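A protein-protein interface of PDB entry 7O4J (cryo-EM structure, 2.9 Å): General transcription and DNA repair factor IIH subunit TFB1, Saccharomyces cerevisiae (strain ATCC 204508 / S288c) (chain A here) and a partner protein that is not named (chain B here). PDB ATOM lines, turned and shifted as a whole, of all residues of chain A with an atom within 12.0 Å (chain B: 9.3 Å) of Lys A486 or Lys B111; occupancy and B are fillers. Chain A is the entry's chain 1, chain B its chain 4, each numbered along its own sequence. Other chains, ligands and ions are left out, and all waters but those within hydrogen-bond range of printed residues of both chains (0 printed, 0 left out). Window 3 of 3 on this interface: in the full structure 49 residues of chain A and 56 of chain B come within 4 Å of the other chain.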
ATOM      1  N   SER A 477      -2.594  18.427  16.461  1.00  0.00           N
ATOM      2  CA  SER A 477      -2.887  18.656  17.870  1.00  0.00           C
ATOM      3  C   SER A 477      -3.024  20.146  18.160  1.00  0.00           C
ATOM      4  O   SER A 477      -3.897  20.560  18.932  1.00  0.00           O
ATOM      5  CB  SER A 477      -1.796  18.035  18.743  1.00  0.00           C
ATOM      6  OG  SER A 477      -2.221  17.930  20.092  1.00  0.00           O
ATOM      7  N   LEU A 478      -2.166  20.967  17.548  1.00  0.00           N
ATOM      8  CA  LEU A 478      -2.226  22.407  17.774  1.00  0.00           C
ATOM      9  C   LEU A 478      -3.545  22.992  17.287  1.00  0.00           C
ATOM     10  O   LEU A 478      -4.203  23.746  18.014  1.00  0.00           O
ATOM     11  CB  LEU A 478      -1.045  23.088  17.082  1.00  0.00           C
ATOM     12  CG  LEU A 478      -0.727  24.525  17.504  1.00  0.00           C
ATOM     13  CD1 LEU A 478       0.721  24.856  17.182  1.00  0.00           C
ATOM     14  CD2 LEU A 478      -1.664  25.519  16.833  1.00  0.00           C
ATOM     15  N   VAL A 479      -3.950  22.661  16.058  1.00  0.00           N
ATOM     16  CA  VAL A 479      -5.226  23.157  15.551  1.00  0.00           C
ATOM     17  C   VAL A 479      -6.378  22.599  16.371  1.00  0.00           C
ATOM     18  O   VAL A 479      -7.366  23.300  16.627  1.00  0.00           O
ATOM     19  CB  VAL A 479      -5.390  22.817  14.057  1.00  0.00           C
ATOM     20  CG1 VAL A 479      -5.358  21.317  13.844  1.00  0.00           C
ATOM     21  CG2 VAL A 479      -6.687  23.398  13.527  1.00  0.00           C
ATOM     22  N   MET A 480      -6.283  21.338  16.794  1.00  0.00           N
ATOM     23  CA  MET A 480      -7.318  20.765  17.646  1.00  0.00           C
ATOM     24  C   MET A 480      -7.432  21.543  18.951  1.00  0.00           C
ATOM     25  O   MET A 480      -8.536  21.857  19.408  1.00  0.00           O
ATOM     26  CB  MET A 480      -7.011  19.292  17.921  1.00  0.00           C
ATOM     27  CG  MET A 480      -7.717  18.324  16.984  1.00  0.00           C
ATOM     28  SD  MET A 480      -9.455  18.082  17.394  1.00  0.00           S
ATOM     29  CE  MET A 480      -9.319  17.277  18.989  1.00  0.00           C
ATOM     30  N   ASP A 481      -6.291  21.865  19.565  1.00  0.00           N
ATOM     31  CA  ASP A 481      -6.307  22.667  20.784  1.00  0.00           C
ATOM     32  C   ASP A 481      -6.832  24.071  20.512  1.00  0.00           C
ATOM     33  O   ASP A 481      -7.602  24.618  21.309  1.00  0.00           O
ATOM     34  CB  ASP A 481      -4.904  22.728  21.387  1.00  0.00           C
ATOM     35  CG  ASP A 481      -4.879  23.424  22.733  1.00  0.00           C
ATOM     36  OD1 ASP A 481      -5.332  22.817  23.726  1.00  0.00           O
ATOM     37  OD2 ASP A 481      -4.407  24.579  22.798  1.00  0.00           O
ATOM     38  N   ASN A 482      -6.424  24.671  19.392  1.00  0.00           N
ATOM     39  CA  ASN A 482      -6.901  26.007  19.055  1.00  0.00           C
ATOM     40  C   ASN A 482      -8.394  26.009  18.755  1.00  0.00           C
ATOM     41  O   ASN A 482      -9.076  27.008  19.010  1.00  0.00           O
ATOM     42  CB  ASN A 482      -6.121  26.554  17.859  1.00  0.00           C
ATOM     43  CG  ASN A 482      -6.291  28.049  17.683  1.00  0.00           C
ATOM     44  OD1 ASN A 482      -7.143  28.669  18.320  1.00  0.00           O
ATOM     45  ND2 ASN A 482      -5.477  28.640  16.815  1.00  0.00           N
ATOM     46  N   LEU A 483      -8.919  24.905  18.219  1.00  0.00           N
ATOM     47  CA  LEU A 483     -10.335  24.844  17.877  1.00  0.00           C
ATOM     48  C   LEU A 483     -11.198  24.552  19.098  1.00  0.00           C
ATOM     49  O   LEU A 483     -12.247  25.180  19.284  1.00  0.00           O
ATOM     50  CB  LEU A 483     -10.563  23.779  16.802  1.00  0.00           C
ATOM     51  CG  LEU A 483     -11.861  23.859  15.995  1.00  0.00           C
ATOM     52  CD1 LEU A 483     -12.036  25.225  15.354  1.00  0.00           C
ATOM     53  CD2 LEU A 483     -11.891  22.767  14.937  1.00  0.00           C
ATOM     54  N   ILE A 484     -10.777  23.607  19.941  1.00  0.00           N
ATOM     55  CA  ILE A 484     -11.580  23.236  21.103  1.00  0.00           C
ATOM     56  C   ILE A 484     -11.687  24.409  22.069  1.00  0.00           C
ATOM     57  O   ILE A 484     -12.759  24.688  22.621  1.00  0.00           O
ATOM     58  CB  ILE A 484     -10.991  21.990  21.793  1.00  0.00           C
ATOM     59  CG1 ILE A 484     -11.845  21.578  22.995  1.00  0.00           C
ATOM     60  CG2 ILE A 484      -9.570  22.256  22.269  1.00  0.00           C
ATOM     61  CD1 ILE A 484     -13.301  21.316  22.666  1.00  0.00           C
ATOM     62  N   ASN A 485     -10.576  25.114  22.290  1.00  0.00           N
ATOM     63  CA  ASN A 485     -10.564  26.201  23.263  1.00  0.00           C
ATOM     64  C   ASN A 485     -11.587  27.271  22.895  1.00  0.00           C
ATOM     65  O   ASN A 485     -12.542  27.520  23.640  1.00  0.00           O
ATOM     66  CB  ASN A 485      -9.159  26.799  23.358  1.00  0.00           C
ATOM     67  CG  ASN A 485      -9.023  27.796  24.494  1.00  0.00           C
ATOM     68  OD1 ASN A 485     -10.002  28.408  24.924  1.00  0.00           O
ATOM     69  ND2 ASN A 485      -7.802  27.962  24.990  1.00  0.00           N
ATOM     70  N   LYS A 486     -11.403  27.914  21.746  1.00  0.00           N
ATOM     71  CA  LYS A 486     -12.323  28.955  21.305  1.00  0.00           C
ATOM     72  C   LYS A 486     -12.053  29.263  19.841  1.00  0.00           C
ATOM     73  O   LYS A 486     -10.986  28.945  19.306  1.00  0.00           O
ATOM     74  CB  LYS A 486     -12.183  30.226  22.155  1.00  0.00           C
ATOM     75  CG  LYS A 486     -13.337  31.229  22.032  1.00  0.00           C
ATOM     76  CD  LYS A 486     -14.727  30.602  22.169  1.00  0.00           C
ATOM     77  CE  LYS A 486     -14.918  29.875  23.496  1.00  0.00           C
ATOM     78  NZ  LYS A 486     -16.025  28.882  23.430  1.00  0.00           N
ATOM     79  N   LEU A 487     -13.039  29.888  19.200  1.00  0.00           N
ATOM     80  CA  LEU A 487     -12.929  30.322  17.812  1.00  0.00           C
ATOM     81  C   LEU A 487     -13.558  31.701  17.700  1.00  0.00           C
ATOM     82  O   LEU A 487     -14.722  31.883  18.068  1.00  0.00           O
ATOM     83  CB  LEU A 487     -13.613  29.333  16.864  1.00  0.00           C
ATOM     84  CG  LEU A 487     -13.480  29.608  15.364  1.00  0.00           C
ATOM     85  CD1 LEU A 487     -13.542  28.306  14.582  1.00  0.00           C
ATOM     86  CD2 LEU A 487     -14.556  30.568  14.877  1.00  0.00           C
ATOM     87  N   ASP A 488     -12.794  32.666  17.193  1.00  0.00           N
ATOM     88  CA  ASP A 488     -13.236  34.052  17.078  1.00  0.00           C
ATOM     89  C   ASP A 488     -13.468  34.365  15.605  1.00  0.00           C
ATOM     90  O   ASP A 488     -12.516  34.430  14.820  1.00  0.00           O
ATOM     91  CB  ASP A 488     -12.207  35.001  17.687  1.00  0.00           C
ATOM     92  CG  ASP A 488     -12.711  36.430  17.783  1.00  0.00           C
ATOM     93  OD1 ASP A 488     -13.655  36.785  17.046  1.00  0.00           O
ATOM     94  OD2 ASP A 488     -12.161  37.200  18.598  1.00  0.00           O
ATOM     95  N   LEU A 489     -14.736  34.558  15.233  1.00  0.00           N
ATOM     96  CA  LEU A 489     -15.056  34.915  13.856  1.00  0.00           C
ATOM     97  C   LEU A 489     -14.742  36.377  13.566  1.00  0.00           C
ATOM     98  O   LEU A 489     -14.411  36.723  12.426  1.00  0.00           O
ATOM     99  CB  LEU A 489     -16.528  34.623  13.569  1.00  0.00           C
ATOM    100  CG  LEU A 489     -16.958  33.154  13.631  1.00  0.00           C
ATOM    101  CD1 LEU A 489     -18.464  33.035  13.455  1.00  0.00           C
ATOM    102  CD2 LEU A 489     -16.236  32.332  12.577  1.00  0.00           C
ATOM    103  N   ASN A 490     -14.842  37.246  14.574  1.00  0.00           N
ATOM    104  CA  ASN A 490     -14.593  38.666  14.360  1.00  0.00           C
ATOM    105  C   ASN A 490     -13.146  38.948  13.976  1.00  0.00           C
ATOM    106  O   ASN A 490     -12.864  40.002  13.398  1.00  0.00           O
ATOM    107  CB  ASN A 490     -14.958  39.457  15.618  1.00  0.00           C
ATOM    108  CG  ASN A 490     -15.308  40.902  15.318  1.00  0.00           C
ATOM    109  OD1 ASN A 490     -15.923  41.204  14.295  1.00  0.00           O
ATOM    110  ND2 ASN A 490     -14.916  41.803  16.211  1.00  0.00           N
ATOM    111  N   GLN A 491     -12.224  38.032  14.284  1.00  0.00           N
ATOM    112  CA  GLN A 491     -10.828  38.236  13.909  1.00  0.00           C
ATOM    113  C   GLN A 491     -10.649  38.223  12.396  1.00  0.00           C
ATOM    114  O   GLN A 491      -9.634  38.709  11.887  1.00  0.00           O
ATOM    115  CB  GLN A 491      -9.957  37.161  14.566  1.00  0.00           C
ATOM    116  CG  GLN A 491      -8.457  37.336  14.352  1.00  0.00           C
ATOM    117  CD  GLN A 491      -7.972  36.771  13.029  1.00  0.00           C
ATOM    118  OE1 GLN A 491      -8.650  35.960  12.399  1.00  0.00           O
ATOM    119  NE2 GLN A 491      -6.793  37.205  12.600  1.00  0.00           N
ATOM    120  N   VAL A 492     -11.629  37.687  11.665  1.00  0.00           N
ATOM    121  CA  VAL A 492     -11.485  37.517  10.222  1.00  0.00           C
ATOM    122  C   VAL A 492     -11.277  38.853   9.522  1.00  0.00           C
ATOM    123  O   VAL A 492     -10.655  38.911   8.454  1.00  0.00           O
ATOM    124  CB  VAL A 492     -12.717  36.778   9.661  1.00  0.00           C
ATOM    125  CG1 VAL A 492     -12.671  36.747   8.150  1.00  0.00           C
ATOM    126  CG2 VAL A 492     -12.789  35.366  10.216  1.00  0.00           C
ATOM    127  N   ILE B  54      -6.919  27.298  10.621  1.00  0.00           N
ATOM    128  CA  ILE B  54      -7.949  27.957  11.417  1.00  0.00           C
ATOM    129  C   ILE B  54      -8.353  29.271  10.763  1.00  0.00           C
ATOM    130  O   ILE B  54      -9.539  29.621  10.719  1.00  0.00           O
ATOM    131  CB  ILE B  54      -7.453  28.174  12.859  1.00  0.00           C
ATOM    132  CG1 ILE B  54      -7.430  26.853  13.633  1.00  0.00           C
ATOM    133  CG2 ILE B  54      -8.327  29.196  13.579  1.00  0.00           C
ATOM    134  CD1 ILE B  54      -8.763  26.123  13.681  1.00  0.00           C
ATOM    135  N   LYS B  55      -7.376  30.018  10.244  1.00  0.00           N
ATOM    136  CA  LYS B  55      -7.682  31.277   9.574  1.00  0.00           C
ATOM    137  C   LYS B  55      -8.593  31.045   8.376  1.00  0.00           C
ATOM    138  O   LYS B  55      -9.559  31.786   8.160  1.00  0.00           O
ATOM    139  CB  LYS B  55      -6.388  31.965   9.139  1.00  0.00           C
ATOM    140  CG  LYS B  55      -6.016  33.188   9.966  1.00  0.00           C
ATOM    141  CD  LYS B  55      -5.827  32.843  11.437  1.00  0.00           C
ATOM    142  CE  LYS B  55      -5.689  34.097  12.284  1.00  0.00           C
ATOM    143  NZ  LYS B  55      -6.016  33.849  13.715  1.00  0.00           N
ATOM    144  N   LEU B  57     -10.535  28.414   8.009  1.00  0.00           N
ATOM    145  CA  LEU B  57     -11.800  27.903   8.529  1.00  0.00           C
ATOM    146  C   LEU B  57     -12.707  29.039   8.985  1.00  0.00           C
ATOM    147  O   LEU B  57     -13.873  29.116   8.579  1.00  0.00           O
ATOM    148  CB  LEU B  57     -11.540  26.932   9.680  1.00  0.00           C
ATOM    149  CG  LEU B  57     -12.581  25.825   9.866  1.00  0.00           C
ATOM    150  CD1 LEU B  57     -12.576  24.861   8.690  1.00  0.00           C
ATOM    151  CD2 LEU B  57     -12.342  25.084  11.173  1.00  0.00           C
ATOM    152  N   GLU B  58     -12.191  29.936   9.827  1.00  0.00           N
ATOM    153  CA  GLU B  58     -12.999  31.061  10.277  1.00  0.00           C
ATOM    154  C   GLU B  58     -13.359  31.994   9.130  1.00  0.00           C
ATOM    155  O   GLU B  58     -14.453  32.567   9.135  1.00  0.00           O
ATOM    156  CB  GLU B  58     -12.272  31.839  11.378  1.00  0.00           C
ATOM    157  CG  GLU B  58     -10.882  32.339  11.002  1.00  0.00           C
ATOM    158  CD  GLU B  58      -9.966  32.501  12.203  1.00  0.00           C
ATOM    159  OE1 GLU B  58      -8.955  33.224  12.083  1.00  0.00           O
ATOM    160  OE2 GLU B  58     -10.253  31.909  13.264  1.00  0.00           O
ATOM    161  N   ASP B 109     -23.850  18.892  21.545  1.00  0.00           N
ATOM    162  CA  ASP B 109     -22.940  19.661  20.704  1.00  0.00           C
ATOM    163  C   ASP B 109     -22.058  20.572  21.550  1.00  0.00           C
ATOM    164  O   ASP B 109     -22.484  21.071  22.591  1.00  0.00           O
ATOM    165  CB  ASP B 109     -23.727  20.487  19.683  1.00  0.00           C
ATOM    166  CG  ASP B 109     -24.600  21.543  20.334  1.00  0.00           C
ATOM    167  OD1 ASP B 109     -24.050  22.519  20.885  1.00  0.00           O
ATOM    168  OD2 ASP B 109     -25.840  21.396  20.292  1.00  0.00           O
ATOM    169  N   LEU B 110     -20.828  20.785  21.095  1.00  0.00           N
ATOM    170  CA  LEU B 110     -19.900  21.650  21.802  1.00  0.00           C
ATOM    171  C   LEU B 110     -20.098  23.102  21.381  1.00  0.00           C
ATOM    172  O   LEU B 110     -20.615  23.403  20.301  1.00  0.00           O
ATOM    173  CB  LEU B 110     -18.456  21.219  21.542  1.00  0.00           C
ATOM    174  CG  LEU B 110     -18.112  19.784  21.951  1.00  0.00           C
ATOM    175  CD1 LEU B 110     -18.278  18.828  20.778  1.00  0.00           C
ATOM    176  CD2 LEU B 110     -16.698  19.710  22.511  1.00  0.00           C
ATOM    177  N   LYS B 111     -19.677  24.012  22.257  1.00  0.00           N
ATOM    178  CA  LYS B 111     -19.818  25.450  22.034  1.00  0.00           C
ATOM    179  C   LYS B 111     -18.488  25.984  21.512  1.00  0.00           C
ATOM    180  O   LYS B 111     -17.494  26.032  22.240  1.00  0.00           O
ATOM    181  CB  LYS B 111     -20.251  26.157  23.316  1.00  0.00           C
ATOM    182  CG  LYS B 111     -19.257  26.054  24.468  1.00  0.00           C
ATOM    183  CD  LYS B 111     -19.905  26.397  25.802  1.00  0.00           C
ATOM    184  CE  LYS B 111     -20.195  27.887  25.925  1.00  0.00           C
ATOM    185  NZ  LYS B 111     -18.992  28.657  26.344  1.00  0.00           N
ATOM    186  N   ILE B 112     -18.473  26.377  20.239  1.00  0.00           N
ATOM    187  CA  ILE B 112     -17.291  26.967  19.620  1.00  0.00           C
ATOM    188  C   ILE B 112     -17.612  28.396  19.205  1.00  0.00           C
ATOM    189  O   ILE B 112     -16.721  29.252  19.143  1.00  0.00           O
ATOM    190  CB  ILE B 112     -16.816  26.140  18.412  1.00  0.00           C
ATOM    191  CG1 ILE B 112     -16.522  24.697  18.833  1.00  0.00           C
ATOM    192  CG2 ILE B 112     -15.589  26.791  17.785  1.00  0.00           C
ATOM    193  CD1 ILE B 112     -17.703  23.764  18.666  1.00  0.00           C
ATOM    194  N   ILE B 113     -18.884  28.659  18.918  1.00  0.00           N
ATOM    195  CA  ILE B 113     -19.353  29.973  18.496  1.00  0.00           C
ATOM    196  C   ILE B 113     -20.479  30.397  19.426  1.00  0.00           C
ATOM    197  O   ILE B 113     -21.329  29.578  19.791  1.00  0.00           O
ATOM    198  CB  ILE B 113     -19.827  29.966  17.029  1.00  0.00           C
ATOM    199  CG1 ILE B 113     -20.905  28.898  16.817  1.00  0.00           C
ATOM    200  CG2 ILE B 113     -18.648  29.735  16.096  1.00  0.00           C
ATOM    201  CD1 ILE B 113     -21.370  28.769  15.380  1.00  0.00           C
ATOM    202  N   ASN B 114     -20.483  31.673  19.807  1.00  0.00           N
ATOM    203  CA  ASN B 114     -21.470  32.173  20.755  1.00  0.00           C
ATOM    204  C   ASN B 114     -22.882  31.936  20.234  1.00  0.00           C
ATOM    205  O   ASN B 114     -23.158  32.095  19.042  1.00  0.00           O
ATOM    206  CB  ASN B 114     -21.249  33.664  21.016  1.00  0.00           C
ATOM    207  CG  ASN B 114     -19.795  34.002  21.273  1.00  0.00           C
ATOM    208  OD1 ASN B 114     -19.028  34.247  20.342  1.00  0.00           O
ATOM    209  ND2 ASN B 114     -19.406  34.016  22.543  1.00  0.00           N
ATOM    210  N   SER B 115     -23.776  31.553  21.142  1.00  0.00           N
ATOM    211  CA  SER B 115     -25.157  31.240  20.800  1.00  0.00           C
ATOM    212  C   SER B 115     -26.017  32.484  20.606  1.00  0.00           C
ATOM    213  O   SER B 115     -27.212  32.351  20.317  1.00  0.00           O
ATOM    214  CB  SER B 115     -25.775  30.352  21.882  1.00  0.00           C
ATOM    215  OG  SER B 115     -27.190  30.399  21.835  1.00  0.00           O
ATOM    216  N   ARG B 122     -25.868  30.275  12.769  1.00  0.00           N
ATOM    217  CA  ARG B 122     -25.279  29.336  13.719  1.00  0.00           C
ATOM    218  C   ARG B 122     -25.623  27.894  13.376  1.00  0.00           C
ATOM    219  O   ARG B 122     -24.782  27.002  13.540  1.00  0.00           O
ATOM    220  CB  ARG B 122     -25.747  29.662  15.135  1.00  0.00           C
ATOM    221  CG  ARG B 122     -24.963  28.949  16.221  1.00  0.00           C
ATOM    222  CD  ARG B 122     -25.325  29.470  17.598  1.00  0.00           C
ATOM    223  NE  ARG B 122     -25.260  28.425  18.616  1.00  0.00           N
ATOM    224  CZ  ARG B 122     -26.182  27.481  18.783  1.00  0.00           C
ATOM    225  NH1 ARG B 122     -26.033  26.573  19.739  1.00  0.00           N
ATOM    226  NH2 ARG B 122     -27.250  27.438  17.998  1.00  0.00           N
ATOM    227  N   ASP B 125     -23.070  26.878  11.013  1.00  0.00           N
ATOM    228  CA  ASP B 125     -21.687  27.047  11.446  1.00  0.00           C
ATOM    229  C   ASP B 125     -21.310  26.057  12.541  1.00  0.00           C
ATOM    230  O   ASP B 125     -20.235  25.450  12.487  1.00  0.00           O
ATOM    231  CB  ASP B 125     -21.461  28.479  11.930  1.00  0.00           C
ATOM    232  CG  ASP B 125     -21.734  29.508  10.853  1.00  0.00           C
ATOM    233  OD1 ASP B 125     -21.568  29.181   9.660  1.00  0.00           O
ATOM    234  OD2 ASP B 125     -22.116  30.646  11.200  1.00  0.00           O
ATOM    235  N   GLU B 126     -22.174  25.882  13.543  1.00  0.00           N
ATOM    236  CA  GLU B 126     -21.836  24.996  14.654  1.00  0.00           C
ATOM    237  C   GLU B 126     -21.650  23.562  14.178  1.00  0.00           C
ATOM    238  O   GLU B 126     -20.715  22.875  14.603  1.00  0.00           O
ATOM    239  CB  GLU B 126     -22.917  25.070  15.731  1.00  0.00           C
ATOM    240  CG  GLU B 126     -22.456  24.580  17.098  1.00  0.00           C
ATOM    241  CD  GLU B 126     -23.209  25.233  18.242  1.00  0.00           C
ATOM    242  OE1 GLU B 126     -23.454  24.549  19.258  1.00  0.00           O
ATOM    243  OE2 GLU B 126     -23.550  26.429  18.130  1.00  0.00           O
ATOM    244  N   VAL B 129     -18.252  23.309  12.288  1.00  0.00           N
ATOM    245  CA  VAL B 129     -17.088  23.201  13.160  1.00  0.00           C
ATOM    246  C   VAL B 129     -17.074  21.860  13.881  1.00  0.00           C
ATOM    247  O   VAL B 129     -16.007  21.270  14.088  1.00  0.00           O
ATOM    248  CB  VAL B 129     -17.054  24.374  14.155  1.00  0.00           C
ATOM    249  CG1 VAL B 129     -15.864  24.238  15.089  1.00  0.00           C
ATOM    250  CG2 VAL B 129     -17.006  25.699  13.410  1.00  0.00           C
ATOM    251  N   GLU B 130     -18.244  21.359  14.284  1.00  0.00           N
ATOM    252  CA  GLU B 130     -18.293  20.070  14.966  1.00  0.00           C
ATOM    253  C   GLU B 130     -17.764  18.955  14.074  1.00  0.00           C
ATOM    254  O   GLU B 130     -17.002  18.095  14.532  1.00  0.00           O
ATOM    255  CB  GLU B 130     -19.724  19.768  15.410  1.00  0.00           C
ATOM    256  CG  GLU B 130     -19.865  18.484  16.214  1.00  0.00           C
ATOM    257  CD  GLU B 130     -21.279  18.262  16.716  1.00  0.00           C
ATOM    258  OE1 GLU B 130     -22.158  19.095  16.410  1.00  0.00           O
ATOM    259  OE2 GLU B 130     -21.511  17.256  17.418  1.00  0.00           O
ATOM    260  N   TYR B 133     -14.129  19.133  13.913  1.00  0.00           N
ATOM    261  CA  TYR B 133     -13.544  18.536  15.109  1.00  0.00           C
ATOM    262  C   TYR B 133     -13.449  17.021  14.970  1.00  0.00           C
ATOM    263  O   TYR B 133     -12.412  16.420  15.273  1.00  0.00           O
ATOM    264  CB  TYR B 133     -14.380  18.914  16.332  1.00  0.00           C
ATOM    265  CG  TYR B 133     -13.710  18.628  17.655  1.00  0.00           C
ATOM    266  CD1 TYR B 133     -12.626  19.381  18.084  1.00  0.00           C
ATOM    267  CD2 TYR B 133     -14.165  17.607  18.478  1.00  0.00           C
ATOM    268  CE1 TYR B 133     -12.014  19.124  19.294  1.00  0.00           C
ATOM    269  CE2 TYR B 133     -13.558  17.342  19.690  1.00  0.00           C
ATOM    270  CZ  TYR B 133     -12.484  18.104  20.093  1.00  0.00           C
ATOM    271  OH  TYR B 133     -11.875  17.844  21.299  1.00  0.00           O
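The backbone carbonyl oxygen (O) of Lys B111 sits at hydrogen-bond distance from the side-chain amino group (NZ) of Lys A486, at 3.4 Å.
OE1 of Glu B58 lies close to OE1 of Gln A491.
The backbone carbonyl oxygen of Leu A487 sits close to the backbone carbonyl oxygen of Ile B112 (3.5 Å).
NZ of Lys B55 lies within salt-bridge range of OE1 of Glu B58, at 3.4 Å.
The side-chain carboxylate of Asp A488 sits at hydrogen-bond distance from the backbone NH of Gln A491 (3.4 Å).
N of Asn A490 sits at hydrogen-bond distance from OD1 of Asp A488 (2.8 Å).
Among the printed residues, pairs that only touch across the chains: Met A480 with Tyr B133 (3.3 Å), Gln A491 with Lys B55 (3.3 Å), Val A479 with Ile B54 (3.4 Å), Val A492 with Glu B58 (3.4 Å), Asp A488 with Glu B58 (3.7 Å), Ile A484 with Leu B110 (3.8 Å), Leu A483 with Ile B54 (3.8 Å), Lys A486 with Ile B112 (3.9 Å), Leu A489 with Glu B58 (3.9 Å), Ile A484 with Tyr B133 (3.9 Å) and Leu A483 with Val B129 (3.96 Å).
Lys A486 touches just these residues of chain B: Lys B111 (3.4 Å) and Ile B112 (3.9 Å).
Lys B111 touches one residue of chain A.
No residue of chain B comes within 4 Å of Asn A485.
Asp B109 touches none of the printed residues of chain A.
Ile B113 touches none of the printed residues of chain A.
No residue of chain A comes within 4 Å of Asn B114.
Printed residues of chain A within 4 Å of Lys B55: Gln A491 (3.3 Å).
Of the printed residues of chain B, Val A479 touches Ile B54.
Of the printed residues of chain A, Glu B58 touches Asp A488 (3.7 Å), Leu A489 (3.9 Å), Gln A491 (2.8 Å) and Val A492 (3.4 Å).
Of the printed residues of chain B, Ile A484 touches Leu B110 and Tyr B133.
Printed residues of chain B within 4 Å of Asp A488: Glu B58 (3.7 Å).
Ser A477 touches none of the printed residues of chain B.
Asn A490 touches none of the printed residues of chain B.
The nearest residue of chain B that does not touch Lys A486 is Ile B113 (5.3 Å).
The nearest printed residue of chain A that does not touch Val B129 is Leu A487 (4.5 Å).
Of the 17 printed residues of chain B, 8 touch a printed residue of chain A.
Of the 16 printed residues of chain A, 10 touch a printed residue of chain B.
Printed residues of chain A that touch a printed residue of chain B: Val A479, Met A480, Leu A483, Ile A484, Lys A486, Leu A487, Asp A488, Leu A489, Gln A491 and Val A492.
Among the printed residues, no Asp or Glu carboxylate lies within 4 Å of a Lys or Arg side-chain nitrogen of the other chain.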
